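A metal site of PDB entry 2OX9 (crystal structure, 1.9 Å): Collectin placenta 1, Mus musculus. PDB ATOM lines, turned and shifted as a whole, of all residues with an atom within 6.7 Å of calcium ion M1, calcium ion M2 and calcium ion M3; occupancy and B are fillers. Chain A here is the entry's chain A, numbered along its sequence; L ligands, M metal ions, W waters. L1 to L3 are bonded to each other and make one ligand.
The side-chain carboxylate (OD1) of Asp 117 binds calcium ion M3, at 2.1 Å. O2 of LG3 L3 is bound to calcium ion M3 (2.3 Å). OD1 of Asn 116 binds calcium ion M3 (2.4 Å). OE1 of Glu 104 is bound to calcium ion M3. Calcium ion M3 is bound by OE1 of Gln 92, at 2.4 Å. Calcium ion M3 is bound by the backbone carbonyl oxygen (O) of Asp 117, at 2.5 Å. Calcium ion M3 is bound by OD1 of Asp 94. Calcium ion M3 is bound by O3 of LG3 L3 (2.7 Å).
OD2 of Asp 117 sits at hydrogen-bond distance from N of Asn 95 (2.7 Å). The side-chain carboxylate (OE1) of Glu 104 lies close to the backbone NH (N) of Trp 96, at 3.1 Å. The backbone carbonyl oxygen (O) of Phe 118 is in hydrogen-bond range of the backbone NH (N) of Asp 105. The side-chain carboxylate (OD2) of Asp 68 lies close to the backbone NH (N) of Ser 73 (2.9 Å). OD1 of Asp 94 sits close to N of Trp 96 (3.4 Å).
Calcium ion M2 is bound by the backbone carbonyl oxygen (O) of Glu 104, the side-chain carboxylate (OE2) of Glu 72, the side-chain carboxylate (OD2) of Asp 68, the side-chain carboxylate (OD1) of Asp 105, the side-chain amide oxygen (OD1) of Asn 95, the side-chain carboxylate (OE1) of Glu 72, water W1 and the side-chain carboxylate (OD1) of Asp 68. Calcium ion M2 has eight donor atoms within binding distance.
Four residues have an atom within 4 Å of calcium ion M1: Glu 72, Asn 95, Pro 102 and Asp 105. The nearest printed residue that does not touch calcium ion M1 is Asp 68 (4.5 Å).
Within 4 Å of calcium ion M2: Asp 68, Glu 72, Asn 95, Glu 104 and Asp 105.
Water W2 binds calcium ion M1, 2.1 Å away. Calcium ion M1 is bound by OE1 of Glu 72, at 2.3 Å. Calcium ion M1 is bound by OD2 of Asp 105, 2.3 Å away. Calcium ion M1 is bound by the backbone carbonyl oxygen (O) of Pro 102 (2.4 Å). The side-chain carboxylate (OD1) of Asp 105 is bound to calcium ion M1, at 2.5 Å. Water W3 is bound to calcium ion M1 (2.5 Å). Calcium ion M1 has six donor atoms within binding distance.
Water W1 lies within hydrogen-bond range of the side-chain carboxylate of Asp 117 (2.7 Å) and the backbone NH of Asn 95 (3.2 Å).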
ATOM      1  N   ASP A  68       4.678 -31.044   3.069  1.00  0.00           N
ATOM      2  CA  ASP A  68       5.382 -30.172   2.135  1.00  0.00           C
ATOM      3  C   ASP A  68       5.513 -28.795   2.795  1.00  0.00           C
ATOM      4  O   ASP A  68       5.421 -27.760   2.134  1.00  0.00           O
ATOM      5  CB  ASP A  68       4.644 -30.096   0.777  1.00  0.00           C
ATOM      6  CG  ASP A  68       3.374 -29.261   0.842  1.00  0.00           C
ATOM      7  OD1 ASP A  68       2.786 -29.136   1.920  1.00  0.00           O
ATOM      8  OD2 ASP A  68       2.961 -28.733  -0.218  1.00  0.00           O
ATOM      9  N   SER A  69       5.727 -28.818   4.106  1.00  0.00           N
ATOM     10  CA  SER A  69       5.894 -27.604   4.907  1.00  0.00           C
ATOM     11  C   SER A  69       7.244 -26.946   4.650  1.00  0.00           C
ATOM     12  O   SER A  69       7.344 -25.724   4.658  1.00  0.00           O
ATOM     13  CB  SER A  69       5.785 -27.924   6.396  1.00  0.00           C
ATOM     14  OG  SER A  69       4.499 -28.409   6.739  1.00  0.00           O
ATOM     15  N   GLN A  71       8.997 -26.905   1.870  1.00  0.00           N
ATOM     16  CA  GLN A  71       8.921 -26.183   0.609  1.00  0.00           C
ATOM     17  C   GLN A  71       7.643 -26.619  -0.109  1.00  0.00           C
ATOM     18  O   GLN A  71       7.514 -27.766  -0.532  1.00  0.00           O
ATOM     19  CB  GLN A  71      10.136 -26.507  -0.255  1.00  0.00           C
ATOM     20  CG  GLN A  71      10.309 -25.585  -1.457  1.00  0.00           C
ATOM     21  CD  GLN A  71      11.595 -25.848  -2.223  1.00  0.00           C
ATOM     22  OE1 GLN A  71      12.687 -25.821  -1.657  1.00  0.00           O
ATOM     23  NE2 GLN A  71      11.469 -26.098  -3.522  1.00  0.00           N
ATOM     24  N   GLU A  72       6.696 -25.697  -0.223  1.00  0.00           N
ATOM     25  CA  GLU A  72       5.423 -25.972  -0.876  1.00  0.00           C
ATOM     26  C   GLU A  72       5.590 -26.815  -2.148  1.00  0.00           C
ATOM     27  O   GLU A  72       6.452 -26.529  -2.984  1.00  0.00           O
ATOM     28  CB  GLU A  72       4.708 -24.658  -1.190  1.00  0.00           C
ATOM     29  CG  GLU A  72       3.303 -24.786  -1.762  1.00  0.00           C
ATOM     30  CD  GLU A  72       2.369 -25.579  -0.860  1.00  0.00           C
ATOM     31  OE1 GLU A  72       2.466 -25.415   0.373  1.00  0.00           O
ATOM     32  OE2 GLU A  72       1.542 -26.344  -1.375  1.00  0.00           O
ATOM     33  N   SER A  73       4.764 -27.850  -2.270  1.00  0.00           N
ATOM     34  CA  SER A  73       4.759 -28.766  -3.409  1.00  0.00           C
ATOM     35  C   SER A  73       5.867 -29.800  -3.443  1.00  0.00           C
ATOM     36  O   SER A  73       5.891 -30.664  -4.313  1.00  0.00           O
ATOM     37  CB  SER A  73       4.740 -27.995  -4.734  1.00  0.00           C
ATOM     38  OG  SER A  73       3.473 -27.395  -4.937  1.00  0.00           O
ATOM     39  N   TRP A  75       6.836 -32.656  -1.569  1.00  0.00           N
ATOM     40  CA  TRP A  75       6.400 -33.624  -0.575  1.00  0.00           C
ATOM     41  C   TRP A  75       7.453 -34.652  -0.185  1.00  0.00           C
ATOM     42  O   TRP A  75       8.054 -35.277  -1.049  1.00  0.00           O
ATOM     43  CB  TRP A  75       5.125 -34.330  -1.056  1.00  0.00           C
ATOM     44  CG  TRP A  75       3.937 -33.422  -1.119  1.00  0.00           C
ATOM     45  CD1 TRP A  75       3.577 -32.619  -2.167  1.00  0.00           C
ATOM     46  CD2 TRP A  75       2.985 -33.182  -0.082  1.00  0.00           C
ATOM     47  NE1 TRP A  75       2.452 -31.903  -1.833  1.00  0.00           N
ATOM     48  CE2 TRP A  75       2.068 -32.228  -0.559  1.00  0.00           C
ATOM     49  CE3 TRP A  75       2.822 -33.688   1.224  1.00  0.00           C
ATOM     50  CZ2 TRP A  75       0.993 -31.765   0.205  1.00  0.00           C
ATOM     51  CZ3 TRP A  75       1.752 -33.227   1.980  1.00  0.00           C
ATOM     52  CH2 TRP A  75       0.856 -32.267   1.476  1.00  0.00           C
ATOM     53  N   GLY A  91      -6.748 -34.332  -8.665  1.00  0.00           N
ATOM     54  CA  GLY A  91      -7.025 -32.956  -8.305  1.00  0.00           C
ATOM     55  C   GLY A  91      -6.249 -32.533  -7.068  1.00  0.00           C
ATOM     56  O   GLY A  91      -6.050 -31.344  -6.821  1.00  0.00           O
ATOM     57  N   GLN A  92      -5.818 -33.526  -6.285  1.00  0.00           N
ATOM     58  CA  GLN A  92      -5.047 -33.268  -5.076  1.00  0.00           C
ATOM     59  C   GLN A  92      -3.570 -33.520  -5.377  1.00  0.00           C
ATOM     60  O   GLN A  92      -3.240 -34.304  -6.252  1.00  0.00           O
ATOM     61  CB  GLN A  92      -5.503 -34.195  -3.950  1.00  0.00           C
ATOM     62  CG  GLN A  92      -6.932 -33.987  -3.546  1.00  0.00           C
ATOM     63  CD  GLN A  92      -7.232 -32.524  -3.298  1.00  0.00           C
ATOM     64  OE1 GLN A  92      -6.614 -31.884  -2.451  1.00  0.00           O
ATOM     65  NE2 GLN A  92      -8.188 -31.986  -4.053  1.00  0.00           N
ATOM     66  N   PRO A  93      -2.658 -32.845  -4.650  1.00  0.00           N
ATOM     67  CA  PRO A  93      -2.883 -31.867  -3.574  1.00  0.00           C
ATOM     68  C   PRO A  93      -3.288 -30.513  -4.144  1.00  0.00           C
ATOM     69  O   PRO A  93      -2.769 -30.090  -5.170  1.00  0.00           O
ATOM     70  CB  PRO A  93      -1.533 -31.827  -2.853  1.00  0.00           C
ATOM     71  CG  PRO A  93      -0.557 -32.118  -3.958  1.00  0.00           C
ATOM     72  CD  PRO A  93      -1.224 -33.212  -4.727  1.00  0.00           C
ATOM     73  N   ASP A  94      -4.229 -29.835  -3.493  1.00  0.00           N
ATOM     74  CA  ASP A  94      -4.691 -28.547  -4.007  1.00  0.00           C
ATOM     75  C   ASP A  94      -4.281 -27.335  -3.177  1.00  0.00           C
ATOM     76  O   ASP A  94      -4.548 -26.203  -3.573  1.00  0.00           O
ATOM     77  CB  ASP A  94      -6.207 -28.581  -4.191  1.00  0.00           C
ATOM     78  CG  ASP A  94      -6.955 -28.815  -2.889  1.00  0.00           C
ATOM     79  OD1 ASP A  94      -6.297 -29.075  -1.865  1.00  0.00           O
ATOM     80  OD2 ASP A  94      -8.204 -28.733  -2.894  1.00  0.00           O
ATOM     81  N   ASN A  95      -3.650 -27.575  -2.030  1.00  0.00           N
ATOM     82  CA  ASN A  95      -3.199 -26.504  -1.134  1.00  0.00           C
ATOM     83  C   ASN A  95      -4.319 -25.485  -0.897  1.00  0.00           C
ATOM     84  O   ASN A  95      -4.096 -24.276  -0.918  1.00  0.00           O
ATOM     85  CB  ASN A  95      -1.974 -25.809  -1.756  1.00  0.00           C
ATOM     86  CG  ASN A  95      -1.047 -25.206  -0.709  1.00  0.00           C
ATOM     87  OD1 ASN A  95      -0.700 -25.860   0.287  1.00  0.00           O
ATOM     88  ND2 ASN A  95      -0.630 -23.967  -0.935  1.00  0.00           N
ATOM     89  N   TRP A  96      -5.515 -25.986  -0.651  1.00  0.00           N
ATOM     90  CA  TRP A  96      -6.697 -25.157  -0.422  1.00  0.00           C
ATOM     91  C   TRP A  96      -6.456 -24.091   0.649  1.00  0.00           C
ATOM     92  O   TRP A  96      -5.897 -24.376   1.705  1.00  0.00           O
ATOM     93  CB  TRP A  96      -7.869 -26.046  -0.013  1.00  0.00           C
ATOM     94  CG  TRP A  96      -9.218 -25.468  -0.260  1.00  0.00           C
ATOM     95  CD1 TRP A  96     -10.141 -25.112   0.678  1.00  0.00           C
ATOM     96  CD2 TRP A  96      -9.824 -25.218  -1.540  1.00  0.00           C
ATOM     97  NE1 TRP A  96     -11.290 -24.656   0.057  1.00  0.00           N
ATOM     98  CE2 TRP A  96     -11.117 -24.711  -1.296  1.00  0.00           C
ATOM     99  CE3 TRP A  96      -9.396 -25.367  -2.866  1.00  0.00           C
ATOM    100  CZ2 TRP A  96     -11.990 -24.367  -2.332  1.00  0.00           C
ATOM    101  CZ3 TRP A  96     -10.262 -25.018  -3.898  1.00  0.00           C
ATOM    102  CH2 TRP A  96     -11.551 -24.523  -3.613  1.00  0.00           C
ATOM    103  N   SER A  98      -4.503 -21.359   0.401  1.00  0.00           N
ATOM    104  CA  SER A  98      -3.170 -20.754   0.391  1.00  0.00           C
ATOM    105  C   SER A  98      -3.235 -19.233   0.319  1.00  0.00           C
ATOM    106  O   SER A  98      -2.286 -18.550   0.703  1.00  0.00           O
ATOM    107  CB  SER A  98      -2.362 -21.275  -0.799  1.00  0.00           C
ATOM    108  OG  SER A  98      -3.011 -20.992  -2.030  1.00  0.00           O
ATOM    109  N   GLY A 101      -3.324 -18.139   4.093  1.00  0.00           N
ATOM    110  CA  GLY A 101      -2.455 -18.809   5.052  1.00  0.00           C
ATOM    111  C   GLY A 101      -1.455 -19.733   4.375  1.00  0.00           C
ATOM    112  O   GLY A 101      -1.189 -19.586   3.179  1.00  0.00           O
ATOM    113  N   PRO A 102      -0.894 -20.713   5.103  1.00  0.00           N
ATOM    114  CA  PRO A 102       0.080 -21.653   4.547  1.00  0.00           C
ATOM    115  C   PRO A 102      -0.513 -22.751   3.669  1.00  0.00           C
ATOM    116  O   PRO A 102       0.218 -23.557   3.083  1.00  0.00           O
ATOM    117  CB  PRO A 102       0.753 -22.218   5.803  1.00  0.00           C
ATOM    118  CG  PRO A 102      -0.385 -22.245   6.768  1.00  0.00           C
ATOM    119  CD  PRO A 102      -1.067 -20.910   6.553  1.00  0.00           C
ATOM    120  N   GLY A 103      -1.849 -22.781   3.594  1.00  0.00           N
ATOM    121  CA  GLY A 103      -2.515 -23.774   2.785  1.00  0.00           C
ATOM    122  C   GLY A 103      -2.640 -25.126   3.464  1.00  0.00           C
ATOM    123  O   GLY A 103      -2.947 -25.208   4.654  1.00  0.00           O
ATOM    124  N   GLU A 104      -2.392 -26.187   2.704  1.00  0.00           N
ATOM    125  CA  GLU A 104      -2.469 -27.562   3.215  1.00  0.00           C
ATOM    126  C   GLU A 104      -1.107 -28.194   3.002  1.00  0.00           C
ATOM    127  O   GLU A 104      -0.681 -28.421   1.867  1.00  0.00           O
ATOM    128  CB  GLU A 104      -3.555 -28.340   2.459  1.00  0.00           C
ATOM    129  CG  GLU A 104      -4.941 -27.680   2.564  1.00  0.00           C
ATOM    130  CD  GLU A 104      -6.055 -28.516   1.967  1.00  0.00           C
ATOM    131  OE1 GLU A 104      -6.038 -28.762   0.742  1.00  0.00           O
ATOM    132  OE2 GLU A 104      -6.957 -28.938   2.720  1.00  0.00           O
ATOM    133  N   ASP A 105      -0.425 -28.515   4.095  1.00  0.00           N
ATOM    134  CA  ASP A 105       0.903 -29.073   3.997  1.00  0.00           C
ATOM    135  C   ASP A 105       1.088 -30.426   4.698  1.00  0.00           C
ATOM    136  O   ASP A 105       2.223 -30.871   4.909  1.00  0.00           O
ATOM    137  CB  ASP A 105       1.918 -28.073   4.572  1.00  0.00           C
ATOM    138  CG  ASP A 105       1.847 -26.710   3.889  1.00  0.00           C
ATOM    139  OD1 ASP A 105       1.139 -26.583   2.861  1.00  0.00           O
ATOM    140  OD2 ASP A 105       2.500 -25.771   4.392  1.00  0.00           O
ATOM    141  N   CYS A 106      -0.020 -31.056   5.060  1.00  0.00           N
ATOM    142  CA  CYS A 106       0.006 -32.336   5.750  1.00  0.00           C
ATOM    143  C   CYS A 106      -0.863 -33.341   4.989  1.00  0.00           C
ATOM    144  O   CYS A 106      -1.960 -33.002   4.579  1.00  0.00           O
ATOM    145  CB  CYS A 106      -0.474 -32.129   7.198  1.00  0.00           C
ATOM    146  SG  CYS A 106       0.794 -31.302   8.231  1.00  0.00           S
ATOM    147  N   ASN A 116      -4.969 -36.990   0.373  1.00  0.00           N
ATOM    148  CA  ASN A 116      -5.426 -35.628   0.275  1.00  0.00           C
ATOM    149  C   ASN A 116      -4.578 -34.772   1.201  1.00  0.00           C
ATOM    150  O   ASN A 116      -4.111 -35.246   2.230  1.00  0.00           O
ATOM    151  CB  ASN A 116      -6.885 -35.513   0.688  1.00  0.00           C
ATOM    152  CG  ASN A 116      -7.313 -34.082   0.867  1.00  0.00           C
ATOM    153  OD1 ASN A 116      -7.127 -33.256  -0.033  1.00  0.00           O
ATOM    154  ND2 ASN A 116      -7.889 -33.775   2.020  1.00  0.00           N
ATOM    155  N   ASP A 117      -4.366 -33.517   0.832  1.00  0.00           N
ATOM    156  CA  ASP A 117      -3.598 -32.621   1.673  1.00  0.00           C
ATOM    157  C   ASP A 117      -4.572 -31.838   2.539  1.00  0.00           C
ATOM    158  O   ASP A 117      -5.605 -31.355   2.054  1.00  0.00           O
ATOM    159  CB  ASP A 117      -2.723 -31.679   0.799  1.00  0.00           C
ATOM    160  CG  ASP A 117      -3.523 -30.921  -0.252  1.00  0.00           C
ATOM    161  OD1 ASP A 117      -4.578 -31.420  -0.707  1.00  0.00           O
ATOM    162  OD2 ASP A 117      -3.082 -29.817  -0.653  1.00  0.00           O
ATOM    163  N   PHE A 118      -4.277 -31.761   3.834  1.00  0.00           N
ATOM    164  CA  PHE A 118      -5.126 -31.048   4.786  1.00  0.00           C
ATOM    165  C   PHE A 118      -4.307 -29.946   5.452  1.00  0.00           C
ATOM    166  O   PHE A 118      -3.075 -29.947   5.399  1.00  0.00           O
ATOM    167  CB  PHE A 118      -5.602 -31.944   5.940  1.00  0.00           C
ATOM    168  CG  PHE A 118      -6.364 -33.169   5.514  1.00  0.00           C
ATOM    169  CD1 PHE A 118      -5.690 -34.312   5.112  1.00  0.00           C
ATOM    170  CD2 PHE A 118      -7.747 -33.211   5.631  1.00  0.00           C
ATOM    171  CE1 PHE A 118      -6.382 -35.481   4.821  1.00  0.00           C
ATOM    172  CE2 PHE A 118      -8.452 -34.382   5.346  1.00  0.00           C
ATOM    173  CZ  PHE A 118      -7.765 -35.522   4.939  1.00  0.00           C
HETATM  174  C1  LIG L   1     -14.030 -33.458  -2.087  1.00  0.00           C
HETATM  175  C2  LIG L   1     -13.996 -33.016  -3.561  1.00  0.00           C
HETATM  176  C3  LIG L   1     -12.786 -32.117  -3.805  1.00  0.00           C
HETATM  177  C4  LIG L   1     -11.511 -32.824  -3.360  1.00  0.00           C
HETATM  178  C5  LIG L   1     -11.630 -33.231  -1.888  1.00  0.00           C
HETATM  179  C6  LIG L   1     -10.410 -34.014  -1.406  1.00  0.00           C
HETATM  180  O1  LIG L   1     -15.183 -32.310  -3.880  1.00  0.00           O
HETATM  181  O2  LIG L   1     -12.706 -31.785  -5.183  1.00  0.00           O
HETATM  182  O3  LIG L   1     -11.298 -33.974  -4.164  1.00  0.00           O
HETATM  183  O4  LIG L   1     -12.797 -34.067  -1.697  1.00  0.00           O
HETATM  184  C1  LG2 L   2     -16.806 -32.773   1.582  1.00  0.00           C
HETATM  185  C2  LG2 L   2     -16.338 -32.496   0.156  1.00  0.00           C
HETATM  186  C3  LG2 L   2     -14.834 -32.717   0.045  1.00  0.00           C
HETATM  187  C4  LG2 L   2     -14.114 -31.855   1.083  1.00  0.00           C
HETATM  188  C5  LG2 L   2     -14.667 -32.151   2.473  1.00  0.00           C
HETATM  189  C6  LG2 L   2     -14.065 -31.241   3.534  1.00  0.00           C
HETATM  190  C7  LG2 L   2     -17.548 -32.861  -1.895  1.00  0.00           C
HETATM  191  C8  LG2 L   2     -18.625 -33.673  -2.587  1.00  0.00           C
HETATM  192  N1  LG2 L   2     -17.052 -33.365  -0.766  1.00  0.00           N
HETATM  193  O1  LG2 L   2     -18.157 -32.490   1.686  1.00  0.00           O
HETATM  194  O2  LG2 L   2     -14.379 -32.374  -1.275  1.00  0.00           O
HETATM  195  O3  LG2 L   2     -12.701 -32.121   1.049  1.00  0.00           O
HETATM  196  O4  LG2 L   2     -16.099 -31.925   2.495  1.00  0.00           O
HETATM  197  O5  LG2 L   2     -14.243 -29.879   3.197  1.00  0.00           O
HETATM  198  O6  LG2 L   2     -17.158 -31.795  -2.389  1.00  0.00           O
HETATM  199  C1  LG3 L   3     -11.866 -31.012   1.033  1.00  0.00           C
HETATM  200  C2  LG3 L   3     -10.451 -31.450   1.414  1.00  0.00           C
HETATM  201  C3  LG3 L   3      -9.479 -30.268   1.292  1.00  0.00           C
HETATM  202  C4  LG3 L   3      -9.600 -29.602  -0.077  1.00  0.00           C
HETATM  203  C5  LG3 L   3     -11.061 -29.271  -0.394  1.00  0.00           C
HETATM  204  C6  LG3 L   3     -11.248 -28.729  -1.804  1.00  0.00           C
HETATM  205  O1  LG3 L   3     -10.447 -31.933   2.742  1.00  0.00           O
HETATM  206  O2  LG3 L   3      -8.160 -30.745   1.479  1.00  0.00           O
HETATM  207  O3  LG3 L   3      -9.076 -30.468  -1.075  1.00  0.00           O
HETATM  208  O4  LG3 L   3     -11.883 -30.457  -0.287  1.00  0.00           O
HETATM  209  O5  LG3 L   3     -12.521 -28.130  -1.962  1.00  0.00           O
HETATM  210 CA    CA M   1       2.324 -24.466   2.477  1.00  0.00          CA
HETATM  211 CA    CA M   2       1.052 -27.536   0.643  1.00  0.00          CA
HETATM  212 CA    CA M   3      -6.559 -30.919  -0.207  1.00  0.00          CA
HETATM  213  O   HOH W   1      -0.715 -28.544  -1.033  1.00  0.00           O
HETATM  214  O   HOH W   2       4.363 -24.971   2.208  1.00  0.00           O
HETATM  215  O   HOH W   3       1.980 -22.512   0.935  1.00  0.00           O
